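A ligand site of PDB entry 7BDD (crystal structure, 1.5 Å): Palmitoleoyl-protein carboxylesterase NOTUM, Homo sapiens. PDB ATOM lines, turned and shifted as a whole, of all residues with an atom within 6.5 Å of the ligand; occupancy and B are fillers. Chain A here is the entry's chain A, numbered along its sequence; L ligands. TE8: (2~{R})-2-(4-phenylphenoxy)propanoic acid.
O04 of the ligand sits at hydrogen-bond distance from N of Trp 51 (2.9 Å).
An oxygen (O04) of the ligand lies within hydrogen-bond range of the backbone NH of Gly 50 (3.0 Å).
N of Ala 156 sits at hydrogen-bond distance from O04 of the ligand (3.0 Å).
OG1 of Thr 159 sits at hydrogen-bond distance from O of Gly 189 (2.9 Å).
N of Val 110 is in hydrogen-bond range of OH of Tyr 105.
O of Trp 51 sits at hydrogen-bond distance from OH of Tyr 105, at 2.6 Å.
The backbone NH (N) of Ala 265 sits at hydrogen-bond distance from the side-chain carboxylate (OD2) of Asp 263, at 2.9 Å.
Tyr 52 touches the ligand.
CG2 of Val 110 touches C18 of the ligand, 3.97 Å away.
Ser 155 touches the ligand (CB to O06, 3.1 Å).
OG1 of Thr 159 touches C09 of the ligand, at 3.4 Å.
O of Ser 188 touches C08 of the ligand, at 3.9 Å.
CE1 of Phe 191 touches C09 of the ligand, at 3.1 Å.
Ile 214 touches the ligand (CD1 to C17, 3.7 Å).
Phe 242 touches the ligand.
Ala 265 touches the ligand.
Hydrophobic or aromatic side chains within 4 Å of the ligand: Trp 51, Tyr 52, Val 110, Ala 156, Phe 191, Ile 214, Phe 242 and Ala 265.
The nearest printed residue that does not touch the ligand is Gly 49 (4.02 Å).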
ATOM      1  N   GLY A  49       8.124 -18.316 -33.501  1.00  0.00           N
ATOM      2  CA  GLY A  49       9.240 -17.543 -33.004  1.00  0.00           C
ATOM      3  C   GLY A  49       9.144 -16.062 -33.339  1.00  0.00           C
ATOM      4  O   GLY A  49       8.100 -15.544 -33.758  1.00  0.00           O
ATOM      5  N   GLY A  50      10.267 -15.354 -33.130  1.00  0.00           N
ATOM      6  CA  GLY A  50      10.346 -13.921 -33.372  1.00  0.00           C
ATOM      7  C   GLY A  50      11.088 -13.091 -32.332  1.00  0.00           C
ATOM      8  O   GLY A  50      10.609 -12.021 -31.941  1.00  0.00           O
ATOM      9  N   TRP A  51      12.279 -13.532 -31.913  1.00  0.00           N
ATOM     10  CA  TRP A  51      13.155 -12.796 -30.960  1.00  0.00           C
ATOM     11  C   TRP A  51      12.385 -12.569 -29.641  1.00  0.00           C
ATOM     12  O   TRP A  51      11.694 -13.492 -29.175  1.00  0.00           O
ATOM     13  CB  TRP A  51      13.796 -11.576 -31.591  1.00  0.00           C
ATOM     14  CG  TRP A  51      14.812 -11.925 -32.656  1.00  0.00           C
ATOM     15  CD1 TRP A  51      14.603 -11.973 -33.998  1.00  0.00           C
ATOM     16  CD2 TRP A  51      16.202 -12.266 -32.447  1.00  0.00           C
ATOM     17  NE1 TRP A  51      15.772 -12.313 -34.655  1.00  0.00           N
ATOM     18  CE2 TRP A  51      16.758 -12.502 -33.720  1.00  0.00           C
ATOM     19  CE3 TRP A  51      17.011 -12.396 -31.323  1.00  0.00           C
ATOM     20  CZ2 TRP A  51      18.103 -12.871 -33.897  1.00  0.00           C
ATOM     21  CZ3 TRP A  51      18.349 -12.763 -31.488  1.00  0.00           C
ATOM     22  CH2 TRP A  51      18.869 -12.999 -32.773  1.00  0.00           C
ATOM     23  N   TYR A  52      12.526 -11.397 -29.010  1.00  0.00           N
ATOM     24  CA  TYR A  52      11.990 -11.085 -27.692  1.00  0.00           C
ATOM     25  C   TYR A  52      12.258  -9.603 -27.438  1.00  0.00           C
ATOM     26  O   TYR A  52      12.927  -8.942 -28.236  1.00  0.00           O
ATOM     27  CB  TYR A  52      12.630 -11.955 -26.598  1.00  0.00           C
ATOM     28  CG  TYR A  52      14.141 -11.861 -26.451  1.00  0.00           C
ATOM     29  CD1 TYR A  52      14.708 -10.939 -25.574  1.00  0.00           C
ATOM     30  CD2 TYR A  52      14.983 -12.704 -27.144  1.00  0.00           C
ATOM     31  CE1 TYR A  52      16.095 -10.855 -25.404  1.00  0.00           C
ATOM     32  CE2 TYR A  52      16.386 -12.624 -26.990  1.00  0.00           C
ATOM     33  CZ  TYR A  52      16.920 -11.704 -26.115  1.00  0.00           C
ATOM     34  OH  TYR A  52      18.290 -11.625 -25.962  1.00  0.00           O
ATOM     35  N   TYR A 105       2.994 -16.374 -31.296  1.00  0.00           N
ATOM     36  CA  TYR A 105       3.909 -15.835 -30.300  1.00  0.00           C
ATOM     37  C   TYR A 105       3.547 -14.366 -30.067  1.00  0.00           C
ATOM     38  O   TYR A 105       3.830 -13.512 -30.919  1.00  0.00           O
ATOM     39  CB  TYR A 105       5.339 -15.966 -30.829  1.00  0.00           C
ATOM     40  CG  TYR A 105       6.481 -15.502 -29.943  1.00  0.00           C
ATOM     41  CD1 TYR A 105       6.486 -15.723 -28.563  1.00  0.00           C
ATOM     42  CD2 TYR A 105       7.602 -14.923 -30.516  1.00  0.00           C
ATOM     43  CE1 TYR A 105       7.560 -15.331 -27.780  1.00  0.00           C
ATOM     44  CE2 TYR A 105       8.680 -14.531 -29.755  1.00  0.00           C
ATOM     45  CZ  TYR A 105       8.663 -14.736 -28.389  1.00  0.00           C
ATOM     46  OH  TYR A 105       9.741 -14.333 -27.637  1.00  0.00           O
ATOM     47  N   VAL A 110      10.353 -15.522 -25.081  1.00  0.00           N
ATOM     48  CA  VAL A 110      10.870 -16.862 -25.405  1.00  0.00           C
ATOM     49  C   VAL A 110      10.003 -17.942 -24.752  1.00  0.00           C
ATOM     50  O   VAL A 110      10.488 -19.027 -24.408  1.00  0.00           O
ATOM     51  CB  VAL A 110      12.364 -17.028 -25.061  1.00  0.00           C
ATOM     52  CG1 VAL A 110      12.958 -18.207 -25.847  1.00  0.00           C
ATOM     53  CG2 VAL A 110      13.178 -15.760 -25.358  1.00  0.00           C
ATOM     54  N   SER A 154       9.800 -23.275 -33.883  1.00  0.00           N
ATOM     55  CA  SER A 154      10.948 -22.790 -34.650  1.00  0.00           C
ATOM     56  C   SER A 154      11.511 -21.507 -34.058  1.00  0.00           C
ATOM     57  O   SER A 154      10.750 -20.614 -33.641  1.00  0.00           O
ATOM     58  CB  SER A 154      10.578 -22.545 -36.128  1.00  0.00           C
ATOM     59  OG  SER A 154      10.201 -23.739 -36.782  1.00  0.00           O
ATOM     60  N   SER A 155      12.842 -21.403 -34.059  1.00  0.00           N
ATOM     61  CA  SER A 155      13.544 -20.192 -33.625  1.00  0.00           C
ATOM     62  C   SER A 155      13.302 -19.931 -32.142  1.00  0.00           C
ATOM     63  O   SER A 155      13.520 -20.828 -31.333  1.00  0.00           O
ATOM     64  CB  SER A 155      13.169 -19.024 -34.542  1.00  0.00           C
ATOM     65  OG  SER A 155      13.395 -19.316 -35.910  1.00  0.00           O
ATOM     66  N   ALA A 156      12.813 -18.745 -31.736  1.00  0.00           N
ATOM     67  CA  ALA A 156      12.483 -18.582 -30.322  1.00  0.00           C
ATOM     68  C   ALA A 156      11.435 -19.599 -29.864  1.00  0.00           C
ATOM     69  O   ALA A 156      11.398 -19.979 -28.676  1.00  0.00           O
ATOM     70  CB  ALA A 156      12.049 -17.139 -30.020  1.00  0.00           C
ATOM     71  N   GLY A 157      10.589 -20.087 -30.779  1.00  0.00           N
ATOM     72  CA  GLY A 157       9.678 -21.176 -30.449  1.00  0.00           C
ATOM     73  C   GLY A 157      10.366 -22.516 -30.226  1.00  0.00           C
ATOM     74  O   GLY A 157       9.874 -23.344 -29.450  1.00  0.00           O
ATOM     75  N   GLY A 158      11.496 -22.761 -30.915  1.00  0.00           N
ATOM     76  CA  GLY A 158      12.286 -23.963 -30.643  1.00  0.00           C
ATOM     77  C   GLY A 158      12.897 -23.947 -29.255  1.00  0.00           C
ATOM     78  O   GLY A 158      12.850 -24.950 -28.532  1.00  0.00           O
ATOM     79  N   THR A 159      13.450 -22.801 -28.840  1.00  0.00           N
ATOM     80  CA  THR A 159      13.901 -22.682 -27.462  1.00  0.00           C
ATOM     81  C   THR A 159      12.719 -22.844 -26.498  1.00  0.00           C
ATOM     82  O   THR A 159      12.846 -23.489 -25.442  1.00  0.00           O
ATOM     83  CB  THR A 159      14.600 -21.328 -27.273  1.00  0.00           C
ATOM     84  OG1 THR A 159      15.576 -21.131 -28.314  1.00  0.00           O
ATOM     85  CG2 THR A 159      15.289 -21.269 -25.912  1.00  0.00           C
ATOM     86  N   SER A 188      15.849 -24.884 -34.793  1.00  0.00           N
ATOM     87  CA  SER A 188      16.548 -23.594 -34.881  1.00  0.00           C
ATOM     88  C   SER A 188      16.525 -22.804 -33.569  1.00  0.00           C
ATOM     89  O   SER A 188      16.538 -21.558 -33.582  1.00  0.00           O
ATOM     90  CB  SER A 188      16.024 -22.772 -36.052  1.00  0.00           C
ATOM     91  OG  SER A 188      16.231 -23.456 -37.299  1.00  0.00           O
ATOM     92  N   GLY A 189      16.530 -23.513 -32.435  1.00  0.00           N
ATOM     93  CA  GLY A 189      16.507 -22.899 -31.120  1.00  0.00           C
ATOM     94  C   GLY A 189      17.668 -23.328 -30.224  1.00  0.00           C
ATOM     95  O   GLY A 189      17.622 -23.139 -28.998  1.00  0.00           O
ATOM     96  N   TRP A 190      18.731 -23.900 -30.835  1.00  0.00           N
ATOM     97  CA  TRP A 190      19.881 -24.495 -30.130  1.00  0.00           C
ATOM     98  C   TRP A 190      21.115 -23.607 -30.318  1.00  0.00           C
ATOM     99  O   TRP A 190      21.841 -23.729 -31.324  1.00  0.00           O
ATOM    100  CB  TRP A 190      20.093 -25.916 -30.662  1.00  0.00           C
ATOM    101  CG  TRP A 190      21.155 -26.798 -29.983  1.00  0.00           C
ATOM    102  CD1 TRP A 190      22.512 -26.806 -30.241  1.00  0.00           C
ATOM    103  CD2 TRP A 190      20.917 -27.852 -29.027  1.00  0.00           C
ATOM    104  NE1 TRP A 190      23.129 -27.784 -29.464  1.00  0.00           N
ATOM    105  CE2 TRP A 190      22.171 -28.431 -28.712  1.00  0.00           C
ATOM    106  CE3 TRP A 190      19.777 -28.336 -28.377  1.00  0.00           C
ATOM    107  CZ2 TRP A 190      22.319 -29.479 -27.796  1.00  0.00           C
ATOM    108  CZ3 TRP A 190      19.911 -29.401 -27.459  1.00  0.00           C
ATOM    109  CH2 TRP A 190      21.175 -29.939 -27.184  1.00  0.00           C
ATOM    110  N   PHE A 191      21.380 -22.714 -29.353  1.00  0.00           N
ATOM    111  CA  PHE A 191      22.395 -21.678 -29.498  1.00  0.00           C
ATOM    112  C   PHE A 191      23.580 -21.907 -28.579  1.00  0.00           C
ATOM    113  O   PHE A 191      23.506 -22.592 -27.557  1.00  0.00           O
ATOM    114  CB  PHE A 191      21.789 -20.292 -29.260  1.00  0.00           C
ATOM    115  CG  PHE A 191      20.911 -19.846 -30.375  1.00  0.00           C
ATOM    116  CD1 PHE A 191      19.597 -20.252 -30.429  1.00  0.00           C
ATOM    117  CD2 PHE A 191      21.413 -19.074 -31.398  1.00  0.00           C
ATOM    118  CE1 PHE A 191      18.801 -19.880 -31.490  1.00  0.00           C
ATOM    119  CE2 PHE A 191      20.616 -18.681 -32.446  1.00  0.00           C
ATOM    120  CZ  PHE A 191      19.302 -19.098 -32.491  1.00  0.00           C
ATOM    121  N   ILE A 214      19.479 -11.409 -22.244  1.00  0.00           N
ATOM    122  CA  ILE A 214      18.603 -12.471 -21.743  1.00  0.00           C
ATOM    123  C   ILE A 214      18.520 -12.437 -20.220  1.00  0.00           C
ATOM    124  O   ILE A 214      17.455 -12.669 -19.637  1.00  0.00           O
ATOM    125  CB  ILE A 214      18.999 -13.845 -22.308  1.00  0.00           C
ATOM    126  CG1 ILE A 214      17.985 -14.911 -21.875  1.00  0.00           C
ATOM    127  CG2 ILE A 214      20.393 -14.246 -21.888  1.00  0.00           C
ATOM    128  CD1 ILE A 214      16.644 -14.774 -22.554  1.00  0.00           C
ATOM    129  N   TRP A 221      10.497 -10.342 -17.125  1.00  0.00           N
ATOM    130  CA  TRP A 221       9.344 -11.174 -17.441  1.00  0.00           C
ATOM    131  C   TRP A 221       8.868 -12.019 -16.266  1.00  0.00           C
ATOM    132  O   TRP A 221       7.791 -12.618 -16.372  1.00  0.00           O
ATOM    133  CB  TRP A 221       9.688 -12.155 -18.557  1.00  0.00           C
ATOM    134  CG  TRP A 221      10.355 -11.594 -19.791  1.00  0.00           C
ATOM    135  CD1 TRP A 221      10.132 -10.371 -20.378  1.00  0.00           C
ATOM    136  CD2 TRP A 221      11.353 -12.246 -20.590  1.00  0.00           C
ATOM    137  NE1 TRP A 221      10.919 -10.237 -21.500  1.00  0.00           N
ATOM    138  CE2 TRP A 221      11.688 -11.379 -21.642  1.00  0.00           C
ATOM    139  CE3 TRP A 221      11.989 -13.496 -20.510  1.00  0.00           C
ATOM    140  CZ2 TRP A 221      12.632 -11.702 -22.612  1.00  0.00           C
ATOM    141  CZ3 TRP A 221      12.947 -13.813 -21.473  1.00  0.00           C
ATOM    142  CH2 TRP A 221      13.262 -12.920 -22.507  1.00  0.00           C
ATOM    143  N   TRP A 239      19.423 -18.075 -16.503  1.00  0.00           N
ATOM    144  CA  TRP A 239      19.670 -17.793 -17.913  1.00  0.00           C
ATOM    145  C   TRP A 239      20.382 -18.933 -18.623  1.00  0.00           C
ATOM    146  O   TRP A 239      20.230 -19.113 -19.837  1.00  0.00           O
ATOM    147  CB  TRP A 239      20.502 -16.493 -18.067  1.00  0.00           C
ATOM    148  CG  TRP A 239      21.939 -16.597 -17.566  1.00  0.00           C
ATOM    149  CD1 TRP A 239      22.402 -16.229 -16.321  1.00  0.00           C
ATOM    150  CD2 TRP A 239      23.082 -17.104 -18.285  1.00  0.00           C
ATOM    151  NE1 TRP A 239      23.757 -16.485 -16.230  1.00  0.00           N
ATOM    152  CE2 TRP A 239      24.198 -17.024 -17.420  1.00  0.00           C
ATOM    153  CE3 TRP A 239      23.273 -17.627 -19.574  1.00  0.00           C
ATOM    154  CZ2 TRP A 239      25.484 -17.434 -17.804  1.00  0.00           C
ATOM    155  CZ3 TRP A 239      24.550 -18.045 -19.945  1.00  0.00           C
ATOM    156  CH2 TRP A 239      25.632 -17.947 -19.069  1.00  0.00           C
ATOM    157  N   PHE A 242      18.409 -21.369 -20.951  1.00  0.00           N
ATOM    158  CA  PHE A 242      17.955 -20.983 -22.288  1.00  0.00           C
ATOM    159  C   PHE A 242      18.900 -21.499 -23.382  1.00  0.00           C
ATOM    160  O   PHE A 242      18.602 -21.343 -24.576  1.00  0.00           O
ATOM    161  CB  PHE A 242      17.819 -19.447 -22.400  1.00  0.00           C
ATOM    162  CG  PHE A 242      16.581 -18.874 -21.732  1.00  0.00           C
ATOM    163  CD1 PHE A 242      15.609 -18.240 -22.480  1.00  0.00           C
ATOM    164  CD2 PHE A 242      16.403 -18.966 -20.353  1.00  0.00           C
ATOM    165  CE1 PHE A 242      14.474 -17.701 -21.874  1.00  0.00           C
ATOM    166  CE2 PHE A 242      15.261 -18.414 -19.743  1.00  0.00           C
ATOM    167  CZ  PHE A 242      14.310 -17.795 -20.520  1.00  0.00           C
ATOM    168  N   PHE A 243      19.996 -22.142 -23.011  1.00  0.00           N
ATOM    169  CA  PHE A 243      20.956 -22.676 -23.965  1.00  0.00           C
ATOM    170  C   PHE A 243      20.774 -24.176 -24.056  1.00  0.00           C
ATOM    171  O   PHE A 243      20.918 -24.895 -23.065  1.00  0.00           O
ATOM    172  CB  PHE A 243      22.382 -22.258 -23.575  1.00  0.00           C
ATOM    173  CG  PHE A 243      22.615 -20.793 -23.791  1.00  0.00           C
ATOM    174  CD1 PHE A 243      22.244 -19.872 -22.831  1.00  0.00           C
ATOM    175  CD2 PHE A 243      23.043 -20.336 -25.024  1.00  0.00           C
ATOM    176  CE1 PHE A 243      22.384 -18.517 -23.054  1.00  0.00           C
ATOM    177  CE2 PHE A 243      23.199 -18.984 -25.263  1.00  0.00           C
ATOM    178  CZ  PHE A 243      22.876 -18.076 -24.275  1.00  0.00           C
ATOM    179  N   ASP A 263      23.995 -21.535 -38.280  1.00  0.00           N
ATOM    180  CA  ASP A 263      22.705 -20.836 -38.230  1.00  0.00           C
ATOM    181  C   ASP A 263      22.905 -19.323 -38.381  1.00  0.00           C
ATOM    182  O   ASP A 263      23.772 -18.728 -37.741  1.00  0.00           O
ATOM    183  CB  ASP A 263      22.040 -21.163 -36.890  1.00  0.00           C
ATOM    184  CG  ASP A 263      20.664 -20.557 -36.764  1.00  0.00           C
ATOM    185  OD1 ASP A 263      19.683 -21.224 -37.142  1.00  0.00           O
ATOM    186  OD2 ASP A 263      20.572 -19.403 -36.291  1.00  0.00           O
ATOM    187  N   ALA A 265      21.095 -16.785 -37.405  1.00  0.00           N
ATOM    188  CA  ALA A 265      20.860 -15.989 -36.202  1.00  0.00           C
ATOM    189  C   ALA A 265      22.029 -16.082 -35.234  1.00  0.00           C
ATOM    190  O   ALA A 265      22.396 -15.081 -34.597  1.00  0.00           O
ATOM    191  CB  ALA A 265      19.552 -16.400 -35.531  1.00  0.00           C
HETATM  192  C10 TE8 L   1      16.605 -17.155 -29.426  1.00  0.00           C
HETATM  193  C13 TE8 L   1      17.035 -17.235 -28.103  1.00  0.00           C
HETATM  194  C15 TE8 L   1      18.449 -18.381 -26.505  1.00  0.00           C
HETATM  195  C17 TE8 L   1      17.205 -16.432 -25.843  1.00  0.00           C
HETATM  196  C01 TE8 L   1      16.247 -15.422 -34.844  1.00  0.00           C
HETATM  197  C02 TE8 L   1      15.130 -16.359 -34.433  1.00  0.00           C
HETATM  198  C03 TE8 L   1      13.772 -15.711 -34.131  1.00  0.00           C
HETATM  199  C07 TE8 L   1      15.862 -17.126 -32.116  1.00  0.00           C
HETATM  200  C08 TE8 L   1      16.076 -18.318 -31.440  1.00  0.00           C
HETATM  201  C09 TE8 L   1      16.445 -18.341 -30.116  1.00  0.00           C
HETATM  202  C11 TE8 L   1      16.408 -15.947 -30.095  1.00  0.00           C
HETATM  203  C12 TE8 L   1      16.025 -15.920 -31.435  1.00  0.00           C
HETATM  204  C14 TE8 L   1      17.936 -18.250 -27.790  1.00  0.00           C
HETATM  205  C16 TE8 L   1      18.077 -17.471 -25.535  1.00  0.00           C
HETATM  206  C18 TE8 L   1      16.692 -16.301 -27.128  1.00  0.00           C
HETATM  207  O04 TE8 L   1      13.156 -16.032 -33.074  1.00  0.00           O
HETATM  208  O05 TE8 L   1      13.270 -14.926 -34.979  1.00  0.00           O
HETATM  209  O06 TE8 L   1      15.500 -17.310 -33.462  1.00  0.00           O
